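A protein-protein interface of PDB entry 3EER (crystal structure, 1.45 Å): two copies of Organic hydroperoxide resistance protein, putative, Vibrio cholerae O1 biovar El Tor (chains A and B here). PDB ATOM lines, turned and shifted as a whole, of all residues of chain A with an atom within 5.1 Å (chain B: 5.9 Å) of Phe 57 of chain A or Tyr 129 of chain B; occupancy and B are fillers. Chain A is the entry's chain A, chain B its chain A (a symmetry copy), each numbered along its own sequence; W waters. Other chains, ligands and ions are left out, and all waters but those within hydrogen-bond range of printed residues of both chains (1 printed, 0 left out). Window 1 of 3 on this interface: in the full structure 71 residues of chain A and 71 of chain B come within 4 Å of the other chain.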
ATOM      1  N   PRO A  53      23.125  -0.853   5.888  1.00  0.00           N
ATOM      2  CA  PRO A  53      23.927  -2.058   5.698  1.00  0.00           C
ATOM      3  C   PRO A  53      24.082  -2.985   6.890  1.00  0.00           C
ATOM      4  O   PRO A  53      24.318  -4.190   6.710  1.00  0.00           O
ATOM      5  CB  PRO A  53      25.286  -1.516   5.241  1.00  0.00           C
ATOM      6  CG  PRO A  53      24.933  -0.182   4.600  1.00  0.00           C
ATOM      7  CD  PRO A  53      23.874   0.363   5.517  1.00  0.00           C
ATOM      8  N   GLU A  54      23.955  -2.458   8.102  1.00  0.00           N
ATOM      9  CA  GLU A  54      24.020  -3.321   9.285  1.00  0.00           C
ATOM     10  C   GLU A  54      22.782  -4.196   9.401  1.00  0.00           C
ATOM     11  O   GLU A  54      22.875  -5.373   9.746  1.00  0.00           O
ATOM     12  CB  GLU A  54      24.283  -2.508  10.546  1.00  0.00           C
ATOM     13  CG  GLU A  54      25.680  -1.933  10.626  1.00  0.00           C
ATOM     14  CD  GLU A  54      25.996  -0.918   9.538  1.00  0.00           C
ATOM     15  OE1 GLU A  54      25.158  -0.020   9.260  1.00  0.00           O
ATOM     16  OE2 GLU A  54      27.084  -1.066   8.944  1.00  0.00           O
ATOM     17  N   GLN A  55      21.613  -3.617   9.127  1.00  0.00           N
ATOM     18  CA  GLN A  55      20.409  -4.396   9.089  1.00  0.00           C
ATOM     19  C   GLN A  55      20.434  -5.426   7.982  1.00  0.00           C
ATOM     20  O   GLN A  55      19.970  -6.566   8.194  1.00  0.00           O
ATOM     21  CB  GLN A  55      19.181  -3.531   8.911  1.00  0.00           C
ATOM     22  CG  GLN A  55      18.855  -2.751  10.160  1.00  0.00           C
ATOM     23  CD  GLN A  55      17.451  -2.188  10.191  1.00  0.00           C
ATOM     24  OE1 GLN A  55      16.853  -1.869   9.167  1.00  0.00           O
ATOM     25  NE2 GLN A  55      16.895  -2.075  11.404  1.00  0.00           N
ATOM     26  N   LEU A  56      20.962  -5.078   6.809  1.00  0.00           N
ATOM     27  CA  LEU A  56      21.047  -6.037   5.726  1.00  0.00           C
ATOM     28  C   LEU A  56      21.925  -7.220   6.103  1.00  0.00           C
ATOM     29  O   LEU A  56      21.604  -8.366   5.819  1.00  0.00           O
ATOM     30  CB  LEU A  56      21.531  -5.343   4.451  1.00  0.00           C
ATOM     31  CG  LEU A  56      20.444  -4.437   3.861  1.00  0.00           C
ATOM     32  CD1 LEU A  56      20.991  -3.354   2.953  1.00  0.00           C
ATOM     33  CD2 LEU A  56      19.387  -5.294   3.091  1.00  0.00           C
ATOM     34  N   PHE A  57      23.041  -6.936   6.772  1.00  0.00           N
ATOM     35  CA  PHE A  57      23.940  -8.000   7.209  1.00  0.00           C
ATOM     36  C   PHE A  57      23.285  -8.854   8.290  1.00  0.00           C
ATOM     37  O   PHE A  57      23.413 -10.068   8.286  1.00  0.00           O
ATOM     38  CB  PHE A  57      25.295  -7.441   7.628  1.00  0.00           C
ATOM     39  CG  PHE A  57      26.347  -8.487   7.775  1.00  0.00           C
ATOM     40  CD1 PHE A  57      26.790  -9.208   6.672  1.00  0.00           C
ATOM     41  CD2 PHE A  57      26.881  -8.760   8.979  1.00  0.00           C
ATOM     42  CE1 PHE A  57      27.754 -10.155   6.796  1.00  0.00           C
ATOM     43  CE2 PHE A  57      27.866  -9.732   9.130  1.00  0.00           C
ATOM     44  CZ  PHE A  57      28.295 -10.426   8.041  1.00  0.00           C
ATOM     45  N   ALA A  58      22.615  -8.226   9.233  1.00  0.00           N
ATOM     46  CA  ALA A  58      21.917  -8.957  10.294  1.00  0.00           C
ATOM     47  C   ALA A  58      20.839  -9.885   9.726  1.00  0.00           C
ATOM     48  O   ALA A  58      20.725 -11.035  10.141  1.00  0.00           O
ATOM     49  CB  ALA A  58      21.280  -7.968  11.272  1.00  0.00           C
ATOM     50  N   VAL A  59      20.039  -9.420   8.767  1.00  0.00           N
ATOM     51  CA  VAL A  59      19.002 -10.237   8.158  1.00  0.00           C
ATOM     52  C   VAL A  59      19.641 -11.410   7.397  1.00  0.00           C
ATOM     53  O   VAL A  59      19.231 -12.569   7.482  1.00  0.00           O
ATOM     54  CB  VAL A  59      18.125  -9.343   7.249  1.00  0.00           C
ATOM     55  CG1 VAL A  59      17.210 -10.168   6.360  1.00  0.00           C
ATOM     56  CG2 VAL A  59      17.311  -8.342   8.095  1.00  0.00           C
ATOM     57  N   GLY A  60      20.686 -11.094   6.631  1.00  0.00           N
ATOM     58  CA  GLY A  60      21.306 -12.120   5.852  1.00  0.00           C
ATOM     59  C   GLY A  60      21.956 -13.182   6.716  1.00  0.00           C
ATOM     60  O   GLY A  60      21.821 -14.377   6.434  1.00  0.00           O
ATOM     61  N   TYR A  61      22.657 -12.773   7.766  1.00  0.00           N
ATOM     62  CA  TYR A  61      23.371 -13.730   8.601  1.00  0.00           C
ATOM     63  C   TYR A  61      22.385 -14.531   9.444  1.00  0.00           C
ATOM     64  O   TYR A  61      22.537 -15.744   9.636  1.00  0.00           O
ATOM     65  CB  TYR A  61      24.414 -13.009   9.466  1.00  0.00           C
ATOM     66  CG  TYR A  61      25.613 -13.831   9.946  1.00  0.00           C
ATOM     67  CD1 TYR A  61      26.751 -13.184  10.465  1.00  0.00           C
ATOM     68  CD2 TYR A  61      25.652 -15.215   9.856  1.00  0.00           C
ATOM     69  CE1 TYR A  61      27.863 -13.889  10.908  1.00  0.00           C
ATOM     70  CE2 TYR A  61      26.765 -15.921  10.273  1.00  0.00           C
ATOM     71  CZ  TYR A  61      27.863 -15.269  10.814  1.00  0.00           C
ATOM     72  OH  TYR A  61      28.977 -15.953  11.259  1.00  0.00           O
ATOM     73  N   ALA A  62      21.357 -13.875   9.976  1.00  0.00           N
ATOM     74  CA  ALA A  62      20.332 -14.617  10.753  1.00  0.00           C
ATOM     75  C   ALA A  62      19.739 -15.754   9.902  1.00  0.00           C
ATOM     76  O   ALA A  62      19.687 -16.906  10.329  1.00  0.00           O
ATOM     77  CB  ALA A  62      19.236 -13.714  11.263  1.00  0.00           C
ATOM     78  N   VAL A  89      24.095  -7.100  14.989  1.00  0.00           N
ATOM     79  CA  VAL A  89      25.188  -6.516  14.249  1.00  0.00           C
ATOM     80  C   VAL A  89      25.382  -5.072  14.700  1.00  0.00           C
ATOM     81  O   VAL A  89      24.440  -4.264  14.655  1.00  0.00           O
ATOM     82  CB  VAL A  89      24.942  -6.587  12.715  1.00  0.00           C
ATOM     83  CG1 VAL A  89      26.042  -5.905  11.948  1.00  0.00           C
ATOM     84  CG2 VAL A  89      24.799  -8.043  12.286  1.00  0.00           C
ATOM     85  N   LEU A 101      32.588  -4.177  11.981  1.00  0.00           N
ATOM     86  CA  LEU A 101      31.350  -4.760  12.475  1.00  0.00           C
ATOM     87  C   LEU A 101      31.617  -5.704  13.649  1.00  0.00           C
ATOM     88  O   LEU A 101      32.647  -6.404  13.731  1.00  0.00           O
ATOM     89  CB  LEU A 101      30.675  -5.590  11.375  1.00  0.00           C
ATOM     90  CG  LEU A 101      30.313  -4.850  10.081  1.00  0.00           C
ATOM     91  CD1 LEU A 101      29.629  -5.818   9.118  1.00  0.00           C
ATOM     92  CD2 LEU A 101      29.463  -3.617  10.347  1.00  0.00           C
ATOM     93  N   VAL A 103      29.438  -8.839  15.674  1.00  0.00           N
ATOM     94  CA  VAL A 103      28.325  -9.739  15.420  1.00  0.00           C
ATOM     95  C   VAL A 103      28.167 -10.686  16.590  1.00  0.00           C
ATOM     96  O   VAL A 103      29.152 -11.284  17.071  1.00  0.00           O
ATOM     97  CB  VAL A 103      28.528 -10.573  14.131  1.00  0.00           C
ATOM     98  CG1 VAL A 103      27.343 -11.500  13.906  1.00  0.00           C
ATOM     99  CG2 VAL A 103      28.788  -9.675  12.939  1.00  0.00           C
ATOM    100  N   TYR A 129      28.512 -17.336   5.506  1.00  0.00           N
ATOM    101  CA  TYR A 129      28.693 -16.074   6.234  1.00  0.00           C
ATOM    102  C   TYR A 129      29.758 -16.224   7.331  1.00  0.00           C
ATOM    103  O   TYR A 129      30.654 -15.392   7.462  1.00  0.00           O
ATOM    104  CB  TYR A 129      27.394 -15.539   6.823  1.00  0.00           C
ATOM    105  CG  TYR A 129      26.513 -14.698   5.948  1.00  0.00           C
ATOM    106  CD1 TYR A 129      26.028 -15.155   4.735  1.00  0.00           C
ATOM    107  CD2 TYR A 129      26.146 -13.435   6.344  1.00  0.00           C
ATOM    108  CE1 TYR A 129      25.166 -14.352   3.956  1.00  0.00           C
ATOM    109  CE2 TYR A 129      25.280 -12.641   5.595  1.00  0.00           C
ATOM    110  CZ  TYR A 129      24.812 -13.081   4.383  1.00  0.00           C
ATOM    111  OH  TYR A 129      23.937 -12.298   3.674  1.00  0.00           O
ATOM    112  N   VAL A 133      33.773 -14.323   7.479  1.00  0.00           N
ATOM    113  CA  VAL A 133      34.211 -13.360   8.503  1.00  0.00           C
ATOM    114  C   VAL A 133      35.159 -13.946   9.538  1.00  0.00           C
ATOM    115  O   VAL A 133      35.663 -13.212  10.386  1.00  0.00           O
ATOM    116  CB  VAL A 133      33.048 -12.684   9.216  1.00  0.00           C
ATOM    117  CG1 VAL A 133      32.105 -12.036   8.192  1.00  0.00           C
ATOM    118  CG2 VAL A 133      32.258 -13.628  10.203  1.00  0.00           C
ATOM    119  N   ILE A 137      36.031 -10.864  12.365  1.00  0.00           N
ATOM    120  CA  ILE A 137      35.000 -10.592  13.365  1.00  0.00           C
ATOM    121  C   ILE A 137      35.003 -11.777  14.338  1.00  0.00           C
ATOM    122  O   ILE A 137      34.926 -12.937  13.930  1.00  0.00           O
ATOM    123  CB  ILE A 137      33.592 -10.468  12.750  1.00  0.00           C
ATOM    124  CG1 ILE A 137      33.543  -9.371  11.667  1.00  0.00           C
ATOM    125  CG2 ILE A 137      32.543 -10.237  13.898  1.00  0.00           C
ATOM    126  CD1 ILE A 137      32.186  -9.165  11.111  1.00  0.00           C
ATOM    127  N   LEU B  56      21.058 -10.357  -0.209  1.00  0.00           N
ATOM    128  CA  LEU B  56      21.171  -9.456   0.922  1.00  0.00           C
ATOM    129  C   LEU B  56      22.599  -8.965   1.096  1.00  0.00           C
ATOM    130  O   LEU B  56      22.840  -7.795   1.361  1.00  0.00           O
ATOM    131  CB  LEU B  56      20.636 -10.136   2.186  1.00  0.00           C
ATOM    132  CG  LEU B  56      19.109 -10.259   2.150  1.00  0.00           C
ATOM    133  CD1 LEU B  56      18.572 -11.344   3.060  1.00  0.00           C
ATOM    134  CD2 LEU B  56      18.450  -8.887   2.510  1.00  0.00           C
ATOM    135  N   PHE B  57      23.560  -9.871   0.923  1.00  0.00           N
ATOM    136  CA  PHE B  57      24.966  -9.497   1.038  1.00  0.00           C
ATOM    137  C   PHE B  57      25.376  -8.570  -0.103  1.00  0.00           C
ATOM    138  O   PHE B  57      26.103  -7.612   0.106  1.00  0.00           O
ATOM    139  CB  PHE B  57      25.857 -10.729   1.155  1.00  0.00           C
ATOM    140  CG  PHE B  57      27.247 -10.414   1.591  1.00  0.00           C
ATOM    141  CD1 PHE B  57      27.494  -9.900   2.859  1.00  0.00           C
ATOM    142  CD2 PHE B  57      28.289 -10.613   0.764  1.00  0.00           C
ATOM    143  CE1 PHE B  57      28.757  -9.620   3.267  1.00  0.00           C
ATOM    144  CE2 PHE B  57      29.592 -10.326   1.160  1.00  0.00           C
ATOM    145  CZ  PHE B  57      29.820  -9.829   2.405  1.00  0.00           C
ATOM    146  N   VAL B  59      23.455  -6.456  -1.814  1.00  0.00           N
ATOM    147  CA  VAL B  59      22.857  -5.149  -1.596  1.00  0.00           C
ATOM    148  C   VAL B  59      23.628  -4.399  -0.497  1.00  0.00           C
ATOM    149  O   VAL B  59      23.964  -3.217  -0.600  1.00  0.00           O
ATOM    150  CB  VAL B  59      21.358  -5.331  -1.254  1.00  0.00           C
ATOM    151  CG1 VAL B  59      20.738  -4.047  -0.731  1.00  0.00           C
ATOM    152  CG2 VAL B  59      20.583  -5.856  -2.480  1.00  0.00           C
ATOM    153  N   GLY B  60      23.920  -5.115   0.589  1.00  0.00           N
ATOM    154  CA  GLY B  60      24.593  -4.477   1.675  1.00  0.00           C
ATOM    155  C   GLY B  60      25.992  -4.028   1.301  1.00  0.00           C
ATOM    156  O   GLY B  60      26.398  -2.914   1.649  1.00  0.00           O
ATOM    157  N   TYR B  61      26.738  -4.871   0.596  1.00  0.00           N
ATOM    158  CA  TYR B  61      28.116  -4.540   0.262  1.00  0.00           C
ATOM    159  C   TYR B  61      28.153  -3.455  -0.808  1.00  0.00           C
ATOM    160  O   TYR B  61      28.979  -2.536  -0.766  1.00  0.00           O
ATOM    161  CB  TYR B  61      28.876  -5.801  -0.173  1.00  0.00           C
ATOM    162  CG  TYR B  61      30.397  -5.794  -0.003  1.00  0.00           C
ATOM    163  CD1 TYR B  61      31.123  -7.000  -0.076  1.00  0.00           C
ATOM    164  CD2 TYR B  61      31.112  -4.636   0.268  1.00  0.00           C
ATOM    165  CE1 TYR B  61      32.502  -7.041   0.076  1.00  0.00           C
ATOM    166  CE2 TYR B  61      32.482  -4.674   0.444  1.00  0.00           C
ATOM    167  CZ  TYR B  61      33.184  -5.865   0.333  1.00  0.00           C
ATOM    168  OH  TYR B  61      34.556  -5.925   0.483  1.00  0.00           O
ATOM    169  N   CYS B  64      27.439  -0.312   1.072  1.00  0.00           N
ATOM    170  CA  CYS B  64      28.479   0.029   2.049  1.00  0.00           C
ATOM    171  C   CYS B  64      29.785   0.407   1.353  1.00  0.00           C
ATOM    172  O   CYS B  64      30.547   1.187   1.866  1.00  0.00           O
ATOM    173  CB  CYS B  64      28.696  -1.094   3.024  1.00  0.00           C
ATOM    174  SG  CYS B  64      29.507  -0.588   4.562  1.00  0.00           S
ATOM    175  N   CYS B 127      36.205   0.328   4.680  1.00  0.00           N
ATOM    176  CA  CYS B 127      34.832  -0.186   4.671  1.00  0.00           C
ATOM    177  C   CYS B 127      34.674  -1.356   5.630  1.00  0.00           C
ATOM    178  O   CYS B 127      35.455  -2.292   5.577  1.00  0.00           O
ATOM    179  CB  CYS B 127      34.501  -0.644   3.272  1.00  0.00           C
ATOM    180  SG  CYS B 127      32.828  -1.270   3.073  1.00  0.00           S
ATOM    181  N   PRO B 128      33.687  -1.340   6.528  1.00  0.00           N
ATOM    182  CA  PRO B 128      33.532  -2.464   7.464  1.00  0.00           C
ATOM    183  C   PRO B 128      33.208  -3.793   6.786  1.00  0.00           C
ATOM    184  O   PRO B 128      33.621  -4.837   7.301  1.00  0.00           O
ATOM    185  CB  PRO B 128      32.411  -1.995   8.410  1.00  0.00           C
ATOM    186  CG  PRO B 128      31.735  -0.918   7.663  1.00  0.00           C
ATOM    187  CD  PRO B 128      32.713  -0.268   6.786  1.00  0.00           C
ATOM    188  N   TYR B 129      32.535  -3.797   5.640  1.00  0.00           N
ATOM    189  CA  TYR B 129      32.314  -5.048   4.903  1.00  0.00           C
ATOM    190  C   TYR B 129      33.642  -5.614   4.378  1.00  0.00           C
ATOM    191  O   TYR B 129      33.928  -6.801   4.530  1.00  0.00           O
ATOM    192  CB  TYR B 129      31.313  -4.894   3.765  1.00  0.00           C
ATOM    193  CG  TYR B 129      29.854  -5.034   4.081  1.00  0.00           C
ATOM    194  CD1 TYR B 129      29.226  -4.243   5.028  1.00  0.00           C
ATOM    195  CD2 TYR B 129      29.087  -5.957   3.413  1.00  0.00           C
ATOM    196  CE1 TYR B 129      27.841  -4.373   5.270  1.00  0.00           C
ATOM    197  CE2 TYR B 129      27.715  -6.081   3.628  1.00  0.00           C
ATOM    198  CZ  TYR B 129      27.092  -5.314   4.579  1.00  0.00           C
ATOM    199  OH  TYR B 129      25.736  -5.429   4.756  1.00  0.00           O
ATOM    200  N   SER B 130      34.487  -4.755   3.807  1.00  0.00           N
ATOM    201  CA  SER B 130      35.817  -5.214   3.371  1.00  0.00           C
ATOM    202  C   SER B 130      36.672  -5.710   4.538  1.00  0.00           C
ATOM    203  O   SER B 130      37.342  -6.733   4.435  1.00  0.00           O
ATOM    204  CB  SER B 130      36.552  -4.069   2.657  1.00  0.00           C
ATOM    205  OG  SER B 130      35.888  -3.730   1.439  1.00  0.00           O
ATOM    206  N   ASN B 131      36.610  -4.992   5.661  1.00  0.00           N
ATOM    207  CA  ASN B 131      37.342  -5.409   6.841  1.00  0.00           C
ATOM    208  C   ASN B 131      36.854  -6.778   7.349  1.00  0.00           C
ATOM    209  O   ASN B 131      37.642  -7.577   7.843  1.00  0.00           O
ATOM    210  CB  ASN B 131      37.285  -4.352   7.941  1.00  0.00           C
ATOM    211  CG  ASN B 131      38.128  -3.117   7.646  1.00  0.00           C
ATOM    212  OD1 ASN B 131      37.752  -1.957   7.977  1.00  0.00           O
ATOM    213  ND2 ASN B 131      39.276  -3.343   7.134  1.00  0.00           N
ATOM    214  N   ALA B 132      35.552  -7.009   7.249  1.00  0.00           N
ATOM    215  CA  ALA B 132      34.971  -8.259   7.735  1.00  0.00           C
ATOM    216  C   ALA B 132      35.442  -9.489   6.976  1.00  0.00           C
ATOM    217  O   ALA B 132      35.601 -10.564   7.567  1.00  0.00           O
ATOM    218  CB  ALA B 132      33.462  -8.176   7.668  1.00  0.00           C
ATOM    219  N   VAL B 133      35.697  -9.334   5.681  1.00  0.00           N
ATOM    220  CA  VAL B 133      35.946 -10.503   4.821  1.00  0.00           C
ATOM    221  C   VAL B 133      37.389 -10.633   4.357  1.00  0.00           C
ATOM    222  O   VAL B 133      37.734 -11.621   3.712  1.00  0.00           O
ATOM    223  CB  VAL B 133      35.025 -10.555   3.610  1.00  0.00           C
ATOM    224  CG1 VAL B 133      33.559 -10.481   4.058  1.00  0.00           C
ATOM    225  CG2 VAL B 133      35.342  -9.469   2.510  1.00  0.00           C
ATOM    226  N   ARG B 134      38.236  -9.665   4.673  1.00  0.00           N
ATOM    227  CA  ARG B 134      39.622  -9.658   4.190  1.00  0.00           C
ATOM    228  C   ARG B 134      40.374 -10.933   4.526  1.00  0.00           C
ATOM    229  O   ARG B 134      40.318 -11.407   5.675  1.00  0.00           O
ATOM    230  CB  ARG B 134      40.385  -8.465   4.774  1.00  0.00           C
ATOM    231  CG  ARG B 134      41.768  -8.282   4.121  1.00  0.00           C
ATOM    232  CD  ARG B 134      42.496  -7.001   4.470  1.00  0.00           C
ATOM    233  NE  ARG B 134      41.645  -5.851   4.201  1.00  0.00           N
ATOM    234  CZ  ARG B 134      41.045  -5.096   5.101  1.00  0.00           C
ATOM    235  NH1 ARG B 134      40.267  -4.086   4.663  1.00  0.00           N
ATOM    236  NH2 ARG B 134      41.216  -5.329   6.418  1.00  0.00           N
HETATM  237  O   HOH W   1      34.197  -5.441  10.021  1.00  0.00           O
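Water W1 lies within hydrogen-bond range of the backbone NH of Leu 101 of chain A (2.8 Å), the backbone carbonyl oxygen of Pro 128 of chain B (2.8 Å) and the backbone NH of Ala 132 of chain B (3.5 Å).
Of the printed residues of chain B, Leu 56 of chain A touches Leu 56, Val 59 and Gly 60.
Phe 57 of chain A touches two residues of chain B.
Of the printed residues of chain B, Tyr 129 of chain A touches Phe 57 (3.5 Å).
Of chain A, only Pro 53 (2.7 Å) and Phe 57 (3.5 Å) come within 4 Å of Tyr 129 of chain B.
Ser 130 of chain B touches none of the printed residues of chain A.
The nearest residue of chain B that does not touch Phe 57 of chain A is Leu 56 of chain B (5.5 Å).
The nearest printed residue of chain B that does not touch Pro 53 of chain A is Gly 60 of chain B (4.01 Å).
N of Tyr 129 of chain B sits close to SG of Cys 127 of chain B, 3.6 Å away.
Among the printed residues, pairs that only touch across the chains: Val 133 of chain A with Ala 132 of chain B (3.3 Å), Phe 57 of chain A with Tyr 129 of chain B (3.5 Å), Tyr 129 of chain A with Phe 57 of chain B (3.5 Å), Phe 57 of chain A with Phe 57 of chain B (3.7 Å), Leu 56 of chain A with Val 59 of chain B (3.8 Å), Leu 56 of chain A with Leu 56 of chain B (3.8 Å), Val 59 of chain A with Leu 56 of chain B (3.8 Å), Ile 137 of chain A with Ala 132 of chain B (3.8 Å), Leu 101 of chain A with Pro 128 of chain B (3.9 Å), Leu 56 of chain A with Gly 60 of chain B (3.98 Å) and Gly 60 of chain A with Leu 56 of chain B (3.98 Å).
Leu 56 of chain A touches Val 59 of chain B, and with the chains exchanged Val 59 of chain A touches Leu 56 of chain B.
Leu 56 of chain A touches Gly 60 of chain B, and with the chains exchanged Gly 60 of chain A touches Leu 56 of chain B.
Phe 57 of chain A touches its own counterpart, Phe 57 of chain B.
Phe 57 of chain A touches Tyr 129 of chain B, and with the chains exchanged Tyr 129 of chain A touches Phe 57 of chain B.
7 positions are printed for both chains.
Of the 12 pairs that touch across the chains among the printed residues, 8 have their exchanged pair printed and touching as well.
OH of Tyr 129 of chain B sits at hydrogen-bond distance from O of Pro 53 of chain A.
Hydrophobic or aromatic side chains of chain B that line the printed part of chain A: Leu 56, Phe 57, Val 59, Pro 128, Tyr 129 and Ala 132.
Hydrophobic or aromatic side chains of chain A within 4 Å of the printed part of chain B: Pro 53, Leu 56, Phe 57, Val 59, Leu 101, Tyr 129, Val 133 and Ile 137.
Among the printed residues, no Asp or Glu carboxylate lies within 4 Å of a Lys or Arg side-chain nitrogen of the other chain.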
